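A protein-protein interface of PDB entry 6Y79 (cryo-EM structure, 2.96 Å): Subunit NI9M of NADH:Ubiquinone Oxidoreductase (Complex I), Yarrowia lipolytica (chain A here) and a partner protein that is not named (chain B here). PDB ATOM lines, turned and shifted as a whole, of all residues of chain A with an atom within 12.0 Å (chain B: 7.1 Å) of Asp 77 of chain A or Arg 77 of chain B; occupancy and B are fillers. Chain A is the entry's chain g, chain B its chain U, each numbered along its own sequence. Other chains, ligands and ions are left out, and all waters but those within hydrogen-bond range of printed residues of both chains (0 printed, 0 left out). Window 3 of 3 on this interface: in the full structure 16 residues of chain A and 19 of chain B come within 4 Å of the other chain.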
ATOM      1  N   LEU A  72      26.940 -14.578  10.974  1.00  0.00           N
ATOM      2  CA  LEU A  72      26.028 -15.697  10.823  1.00  0.00           C
ATOM      3  C   LEU A  72      25.376 -15.980  12.161  1.00  0.00           C
ATOM      4  O   LEU A  72      26.068 -16.164  13.167  1.00  0.00           O
ATOM      5  CB  LEU A  72      26.769 -16.927  10.343  1.00  0.00           C
ATOM      6  CG  LEU A  72      27.434 -16.725   8.997  1.00  0.00           C
ATOM      7  CD1 LEU A  72      28.383 -17.869   8.881  1.00  0.00           C
ATOM      8  CD2 LEU A  72      26.389 -16.746   7.892  1.00  0.00           C
ATOM      9  N   THR A  73      24.049 -16.022  12.162  1.00  0.00           N
ATOM     10  CA  THR A  73      23.279 -16.278  13.372  1.00  0.00           C
ATOM     11  C   THR A  73      23.050 -17.785  13.477  1.00  0.00           C
ATOM     12  O   THR A  73      22.059 -18.357  13.016  1.00  0.00           O
ATOM     13  CB  THR A  73      21.987 -15.475  13.351  1.00  0.00           C
ATOM     14  OG1 THR A  73      22.313 -14.091  13.206  1.00  0.00           O
ATOM     15  CG2 THR A  73      21.200 -15.660  14.642  1.00  0.00           C
ATOM     16  N   GLY A  74      24.041 -18.438  14.062  1.00  0.00           N
ATOM     17  CA  GLY A  74      23.990 -19.854  14.316  1.00  0.00           C
ATOM     18  C   GLY A  74      25.070 -20.224  15.289  1.00  0.00           C
ATOM     19  O   GLY A  74      26.194 -19.738  15.168  1.00  0.00           O
ATOM     20  N   PHE A  75      24.710 -21.074  16.250  1.00  0.00           N
ATOM     21  CA  PHE A  75      25.551 -21.466  17.383  1.00  0.00           C
ATOM     22  C   PHE A  75      26.024 -20.239  18.163  1.00  0.00           C
ATOM     23  O   PHE A  75      27.189 -20.128  18.551  1.00  0.00           O
ATOM     24  CB  PHE A  75      26.703 -22.377  16.910  1.00  0.00           C
ATOM     25  CG  PHE A  75      26.219 -23.677  16.304  1.00  0.00           C
ATOM     26  CD1 PHE A  75      25.882 -23.767  14.956  1.00  0.00           C
ATOM     27  CD2 PHE A  75      26.037 -24.794  17.104  1.00  0.00           C
ATOM     28  CE1 PHE A  75      25.396 -24.954  14.420  1.00  0.00           C
ATOM     29  CE2 PHE A  75      25.557 -25.987  16.564  1.00  0.00           C
ATOM     30  CZ  PHE A  75      25.236 -26.060  15.223  1.00  0.00           C
ATOM     31  N   ASP A  76      25.076 -19.314  18.390  1.00  0.00           N
ATOM     32  CA  ASP A  76      25.369 -18.109  19.158  1.00  0.00           C
ATOM     33  C   ASP A  76      25.714 -18.449  20.603  1.00  0.00           C
ATOM     34  O   ASP A  76      26.458 -17.707  21.249  1.00  0.00           O
ATOM     35  CB  ASP A  76      24.184 -17.150  19.140  1.00  0.00           C
ATOM     36  CG  ASP A  76      23.801 -16.702  17.743  1.00  0.00           C
ATOM     37  OD1 ASP A  76      24.684 -16.541  16.869  1.00  0.00           O
ATOM     38  OD2 ASP A  76      22.588 -16.550  17.523  1.00  0.00           O
ATOM     39  N   ASP A  77      25.169 -19.544  21.139  1.00  0.00           N
ATOM     40  CA  ASP A  77      25.534 -20.036  22.482  1.00  0.00           C
ATOM     41  C   ASP A  77      27.030 -20.251  22.652  1.00  0.00           C
ATOM     42  O   ASP A  77      27.746 -20.520  21.676  1.00  0.00           O
ATOM     43  CB  ASP A  77      24.829 -21.342  22.770  1.00  0.00           C
ATOM     44  CG  ASP A  77      25.069 -22.380  21.670  1.00  0.00           C
ATOM     45  OD1 ASP A  77      24.598 -22.134  20.555  1.00  0.00           O
ATOM     46  OD2 ASP A  77      25.755 -23.364  21.963  1.00  0.00           O
ATOM     47  N   PRO B  23      34.729 -19.498  27.453  1.00  0.00           N
ATOM     48  CA  PRO B  23      33.767 -20.471  27.946  1.00  0.00           C
ATOM     49  C   PRO B  23      34.161 -21.900  27.603  1.00  0.00           C
ATOM     50  O   PRO B  23      35.085 -22.162  26.833  1.00  0.00           O
ATOM     51  CB  PRO B  23      32.462 -20.078  27.255  1.00  0.00           C
ATOM     52  CG  PRO B  23      32.630 -18.634  26.937  1.00  0.00           C
ATOM     53  CD  PRO B  23      34.080 -18.466  26.608  1.00  0.00           C
ATOM     54  N   ASP B  24      33.442 -22.829  28.224  1.00  0.00           N
ATOM     55  CA  ASP B  24      33.588 -24.244  27.928  1.00  0.00           C
ATOM     56  C   ASP B  24      33.114 -24.537  26.510  1.00  0.00           C
ATOM     57  O   ASP B  24      32.202 -23.888  25.989  1.00  0.00           O
ATOM     58  CB  ASP B  24      32.788 -25.088  28.922  1.00  0.00           C
ATOM     59  CG  ASP B  24      33.345 -25.025  30.340  1.00  0.00           C
ATOM     60  OD1 ASP B  24      34.571 -24.870  30.503  1.00  0.00           O
ATOM     61  OD2 ASP B  24      32.546 -25.126  31.298  1.00  0.00           O
ATOM     62  N   VAL B  25      33.795 -25.490  25.873  1.00  0.00           N
ATOM     63  CA  VAL B  25      33.423 -26.070  24.586  1.00  0.00           C
ATOM     64  C   VAL B  25      33.608 -27.577  24.727  1.00  0.00           C
ATOM     65  O   VAL B  25      34.663 -28.023  25.189  1.00  0.00           O
ATOM     66  CB  VAL B  25      34.300 -25.553  23.425  1.00  0.00           C
ATOM     67  CG1 VAL B  25      33.851 -26.153  22.110  1.00  0.00           C
ATOM     68  CG2 VAL B  25      34.326 -24.027  23.335  1.00  0.00           C
ATOM     69  N   VAL B  26      32.594 -28.369  24.359  1.00  0.00           N
ATOM     70  CA  VAL B  26      32.749 -29.825  24.423  1.00  0.00           C
ATOM     71  C   VAL B  26      33.296 -30.356  23.108  1.00  0.00           C
ATOM     72  O   VAL B  26      33.067 -29.786  22.039  1.00  0.00           O
ATOM     73  CB  VAL B  26      31.441 -30.534  24.815  1.00  0.00           C
ATOM     74  CG1 VAL B  26      31.022 -30.131  26.215  1.00  0.00           C
ATOM     75  CG2 VAL B  26      30.324 -30.312  23.795  1.00  0.00           C
ATOM     76  N   VAL B  28      35.116 -33.127  20.133  1.00  0.00           N
ATOM     77  CA  VAL B  28      34.755 -34.205  19.222  1.00  0.00           C
ATOM     78  C   VAL B  28      35.396 -35.487  19.720  1.00  0.00           C
ATOM     79  O   VAL B  28      36.610 -35.544  19.939  1.00  0.00           O
ATOM     80  CB  VAL B  28      35.187 -33.886  17.784  1.00  0.00           C
ATOM     81  CG1 VAL B  28      34.933 -35.078  16.874  1.00  0.00           C
ATOM     82  CG2 VAL B  28      34.419 -32.702  17.282  1.00  0.00           C
ATOM     83  N   CYS B  46      28.599 -27.523   7.900  1.00  0.00           N
ATOM     84  CA  CYS B  46      29.433 -26.517   8.546  1.00  0.00           C
ATOM     85  C   CYS B  46      30.366 -25.797   7.583  1.00  0.00           C
ATOM     86  O   CYS B  46      31.471 -25.424   7.980  1.00  0.00           O
ATOM     87  CB  CYS B  46      30.257 -27.151   9.660  1.00  0.00           C
ATOM     88  SG  CYS B  46      29.307 -27.815  11.013  1.00  0.00           S
ATOM     89  N   LYS B  70      36.724 -17.781  19.286  1.00  0.00           N
ATOM     90  CA  LYS B  70      35.269 -17.736  19.386  1.00  0.00           C
ATOM     91  C   LYS B  70      34.600 -18.483  18.241  1.00  0.00           C
ATOM     92  O   LYS B  70      33.480 -18.979  18.395  1.00  0.00           O
ATOM     93  CB  LYS B  70      34.797 -16.282  19.433  1.00  0.00           C
ATOM     94  CG  LYS B  70      33.370 -16.072  19.914  1.00  0.00           C
ATOM     95  CD  LYS B  70      32.434 -15.760  18.758  1.00  0.00           C
ATOM     96  CE  LYS B  70      32.741 -14.406  18.150  1.00  0.00           C
ATOM     97  NZ  LYS B  70      31.876 -14.136  16.970  1.00  0.00           N
ATOM     98  N   GLU B  71      35.271 -18.592  17.098  1.00  0.00           N
ATOM     99  CA  GLU B  71      34.728 -19.309  15.952  1.00  0.00           C
ATOM    100  C   GLU B  71      35.263 -20.724  15.833  1.00  0.00           C
ATOM    101  O   GLU B  71      34.580 -21.597  15.283  1.00  0.00           O
ATOM    102  CB  GLU B  71      35.024 -18.524  14.682  1.00  0.00           C
ATOM    103  CG  GLU B  71      34.570 -17.098  14.822  1.00  0.00           C
ATOM    104  CD  GLU B  71      34.842 -16.287  13.601  1.00  0.00           C
ATOM    105  OE1 GLU B  71      35.711 -16.698  12.815  1.00  0.00           O
ATOM    106  OE2 GLU B  71      34.193 -15.234  13.430  1.00  0.00           O
ATOM    107  N   GLY B  72      36.456 -20.969  16.372  1.00  0.00           N
ATOM    108  CA  GLY B  72      36.896 -22.324  16.635  1.00  0.00           C
ATOM    109  C   GLY B  72      36.038 -23.047  17.651  1.00  0.00           C
ATOM    110  O   GLY B  72      36.012 -24.280  17.666  1.00  0.00           O
ATOM    111  N   ARG B  73      35.364 -22.302  18.524  1.00  0.00           N
ATOM    112  CA  ARG B  73      34.285 -22.847  19.338  1.00  0.00           C
ATOM    113  C   ARG B  73      33.142 -23.380  18.475  1.00  0.00           C
ATOM    114  O   ARG B  73      32.716 -24.539  18.606  1.00  0.00           O
ATOM    115  CB  ARG B  73      33.807 -21.738  20.268  1.00  0.00           C
ATOM    116  CG  ARG B  73      32.471 -21.912  20.922  1.00  0.00           C
ATOM    117  CD  ARG B  73      32.309 -20.851  22.001  1.00  0.00           C
ATOM    118  NE  ARG B  73      33.532 -20.708  22.789  1.00  0.00           N
ATOM    119  CZ  ARG B  73      34.191 -19.564  22.950  1.00  0.00           C
ATOM    120  NH1 ARG B  73      33.741 -18.452  22.388  1.00  0.00           N
ATOM    121  NH2 ARG B  73      35.299 -19.535  23.673  1.00  0.00           N
ATOM    122  N   ARG B  74      32.651 -22.539  17.564  1.00  0.00           N
ATOM    123  CA  ARG B  74      31.426 -22.854  16.842  1.00  0.00           C
ATOM    124  C   ARG B  74      31.630 -23.932  15.787  1.00  0.00           C
ATOM    125  O   ARG B  74      30.692 -24.689  15.508  1.00  0.00           O
ATOM    126  CB  ARG B  74      30.854 -21.586  16.220  1.00  0.00           C
ATOM    127  CG  ARG B  74      30.473 -20.559  17.258  1.00  0.00           C
ATOM    128  CD  ARG B  74      29.736 -19.395  16.651  1.00  0.00           C
ATOM    129  NE  ARG B  74      30.534 -18.717  15.646  1.00  0.00           N
ATOM    130  CZ  ARG B  74      30.278 -17.495  15.200  1.00  0.00           C
ATOM    131  NH1 ARG B  74      31.059 -16.947  14.280  1.00  0.00           N
ATOM    132  NH2 ARG B  74      29.242 -16.823  15.680  1.00  0.00           N
ATOM    133  N   VAL B  75      32.837 -24.048  15.216  1.00  0.00           N
ATOM    134  CA  VAL B  75      33.064 -25.122  14.244  1.00  0.00           C
ATOM    135  C   VAL B  75      33.044 -26.486  14.935  1.00  0.00           C
ATOM    136  O   VAL B  75      32.479 -27.457  14.405  1.00  0.00           O
ATOM    137  CB  VAL B  75      34.360 -24.891  13.431  1.00  0.00           C
ATOM    138  CG1 VAL B  75      34.265 -23.610  12.666  1.00  0.00           C
ATOM    139  CG2 VAL B  75      35.616 -24.866  14.287  1.00  0.00           C
ATOM    140  N   THR B  76      33.570 -26.558  16.161  1.00  0.00           N
ATOM    141  CA  THR B  76      33.562 -27.806  16.910  1.00  0.00           C
ATOM    142  C   THR B  76      32.150 -28.163  17.339  1.00  0.00           C
ATOM    143  O   THR B  76      31.730 -29.325  17.224  1.00  0.00           O
ATOM    144  CB  THR B  76      34.482 -27.685  18.123  1.00  0.00           C
ATOM    145  OG1 THR B  76      35.817 -27.428  17.680  1.00  0.00           O
ATOM    146  CG2 THR B  76      34.474 -28.954  18.947  1.00  0.00           C
ATOM    147  N   ARG B  77      31.382 -27.162  17.776  1.00  0.00           N
ATOM    148  CA  ARG B  77      30.017 -27.428  18.223  1.00  0.00           C
ATOM    149  C   ARG B  77      29.111 -27.842  17.069  1.00  0.00           C
ATOM    150  O   ARG B  77      28.276 -28.746  17.227  1.00  0.00           O
ATOM    151  CB  ARG B  77      29.461 -26.207  18.941  1.00  0.00           C
ATOM    152  CG  ARG B  77      30.177 -25.941  20.237  1.00  0.00           C
ATOM    153  CD  ARG B  77      29.651 -24.719  20.927  1.00  0.00           C
ATOM    154  NE  ARG B  77      30.302 -24.529  22.215  1.00  0.00           N
ATOM    155  CZ  ARG B  77      30.121 -23.464  22.981  1.00  0.00           C
ATOM    156  NH1 ARG B  77      29.316 -22.496  22.577  1.00  0.00           N
ATOM    157  NH2 ARG B  77      30.755 -23.359  24.140  1.00  0.00           N
ATOM    158  N   CYS B  78      29.288 -27.243  15.887  1.00  0.00           N
ATOM    159  CA  CYS B  78      28.451 -27.640  14.762  1.00  0.00           C
ATOM    160  C   CYS B  78      28.827 -29.020  14.237  1.00  0.00           C
ATOM    161  O   CYS B  78      27.937 -29.786  13.833  1.00  0.00           O
ATOM    162  CB  CYS B  78      28.518 -26.596  13.653  1.00  0.00           C
ATOM    163  SG  CYS B  78      29.946 -26.702  12.593  1.00  0.00           S
ATOM    164  N   ALA B  79      30.116 -29.379  14.266  1.00  0.00           N
ATOM    165  CA  ALA B  79      30.473 -30.740  13.876  1.00  0.00           C
ATOM    166  C   ALA B  79      29.937 -31.777  14.859  1.00  0.00           C
ATOM    167  O   ALA B  79      29.483 -32.844  14.431  1.00  0.00           O
ATOM    168  CB  ALA B  79      31.983 -30.870  13.734  1.00  0.00           C
ATOM    169  N   VAL B  80      29.946 -31.467  16.164  1.00  0.00           N
ATOM    170  CA  VAL B  80      29.352 -32.353  17.169  1.00  0.00           C
ATOM    171  C   VAL B  80      27.852 -32.521  16.925  1.00  0.00           C
ATOM    172  O   VAL B  80      27.295 -33.626  17.080  1.00  0.00           O
ATOM    173  CB  VAL B  80      29.657 -31.811  18.581  1.00  0.00           C
ATOM    174  CG1 VAL B  80      28.748 -32.403  19.645  1.00  0.00           C
ATOM    175  CG2 VAL B  80      31.100 -32.087  18.947  1.00  0.00           C
ATOM    176  N   SER B  81      27.184 -31.434  16.504  1.00  0.00           N
ATOM    177  CA  SER B  81      25.764 -31.512  16.172  1.00  0.00           C
ATOM    178  C   SER B  81      25.518 -32.473  15.017  1.00  0.00           C
ATOM    179  O   SER B  81      24.607 -33.312  15.086  1.00  0.00           O
ATOM    180  CB  SER B  81      25.217 -30.127  15.833  1.00  0.00           C
ATOM    181  OG  SER B  81      25.689 -29.687  14.575  1.00  0.00           O
ATOM    182  N   VAL B  82      26.361 -32.403  13.977  1.00  0.00           N
ATOM    183  CA  VAL B  82      26.239 -33.324  12.839  1.00  0.00           C
ATOM    184  C   VAL B  82      26.467 -34.772  13.277  1.00  0.00           C
ATOM    185  O   VAL B  82      25.743 -35.680  12.855  1.00  0.00           O
ATOM    186  CB  VAL B  82      27.200 -32.932  11.701  1.00  0.00           C
ATOM    187  CG1 VAL B  82      27.028 -33.856  10.508  1.00  0.00           C
ATOM    188  CG2 VAL B  82      26.949 -31.522  11.264  1.00  0.00           C
ATOM    189  N   ILE B  83      27.443 -35.005  14.160  1.00  0.00           N
ATOM    190  CA  ILE B  83      27.774 -36.392  14.507  1.00  0.00           C
ATOM    191  C   ILE B  83      26.696 -37.042  15.385  1.00  0.00           C
ATOM    192  O   ILE B  83      26.353 -38.208  15.181  1.00  0.00           O
ATOM    193  CB  ILE B  83      29.166 -36.486  15.165  1.00  0.00           C
ATOM    194  CG1 ILE B  83      30.246 -35.948  14.234  1.00  0.00           C
ATOM    195  CG2 ILE B  83      29.550 -37.926  15.481  1.00  0.00           C
ATOM    196  CD1 ILE B  83      30.235 -36.566  12.870  1.00  0.00           C
ATOM    197  N   GLU B  84      26.100 -36.320  16.339  1.00  0.00           N
ATOM    198  CA  GLU B  84      25.018 -36.936  17.121  1.00  0.00           C
ATOM    199  C   GLU B  84      23.725 -37.044  16.319  1.00  0.00           C
ATOM    200  O   GLU B  84      22.935 -37.973  16.532  1.00  0.00           O
ATOM    201  CB  GLU B  84      24.754 -36.163  18.404  1.00  0.00           C
ATOM    202  CG  GLU B  84      25.964 -36.007  19.263  1.00  0.00           C
ATOM    203  CD  GLU B  84      25.736 -35.032  20.393  1.00  0.00           C
ATOM    204  OE1 GLU B  84      26.282 -35.245  21.498  1.00  0.00           O
ATOM    205  OE2 GLU B  84      24.978 -34.070  20.175  1.00  0.00           O
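The side-chain carboxylate (OD2) of Asp 77 of chain A is in salt-bridge range of the guanidinium group (NH1) of Arg 77 of chain B (3.7 Å).
Asp 77 of chain A touches just one residue of chain B: Arg 77 (2.7 Å).
Arg 77 of chain B touches two residues of chain A.
No residue of chain A comes within 4 Å of Pro 23 of chain B.
No residue of chain A comes within 4 Å of Asp 24 of chain B.
No residue of chain A comes within 4 Å of Val 25 of chain B.
No residue of chain A comes within 4 Å of Arg 73 of chain B.
Ser 81 of chain B touches one residue of chain A.
Of the printed residues of chain A, Arg 74 of chain B touches Gly 74 (3.9 Å) and Phe 75 (3.3 Å).
Printed residues of chain B within 4 Å of Phe 75 of chain A: Arg 74, Arg 77, Cys 78 and Ser 81.
Of the printed residues of chain B, Gly 74 of chain A touches Arg 74.
The guanidinium group of Arg 77 of chain B sits at hydrogen-bond distance from the backbone carbonyl oxygen of Asp 24 of chain B.
The guanidinium group (NH1) of Arg 74 of chain B lies within salt-bridge range of the side-chain carboxylate (OE2) of Glu 71 of chain B, at 3.7 Å.
N of Gly 74 of chain A sits at hydrogen-bond distance from OD1 of Asp 76 of chain A, at 3.4 Å.
SG of Cys 46 of chain B forms a disulfide with SG of Cys 78 of chain B, at 2.0 Å.
O of Gly 74 of chain A touches CD of Arg 74 of chain B, at 3.9 Å.
Phe 75 of chain A touches Arg 74 of chain B.
Phe 75 of chain A touches Arg 77 of chain B (CE2 to O, 3.9 Å).
CE1 of Phe 75 of chain A touches CB of Cys 78 of chain B, at 3.6 Å.
Phe 75 of chain A touches Ser 81 of chain B.
Of the 6 printed residues of chain A, 3 touch a printed residue of chain B.
Printed residues of chain A that touch a printed residue of chain B: Gly 74, Phe 75 and Asp 77.
Among the printed residues, 6 pairs touch across the chains.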
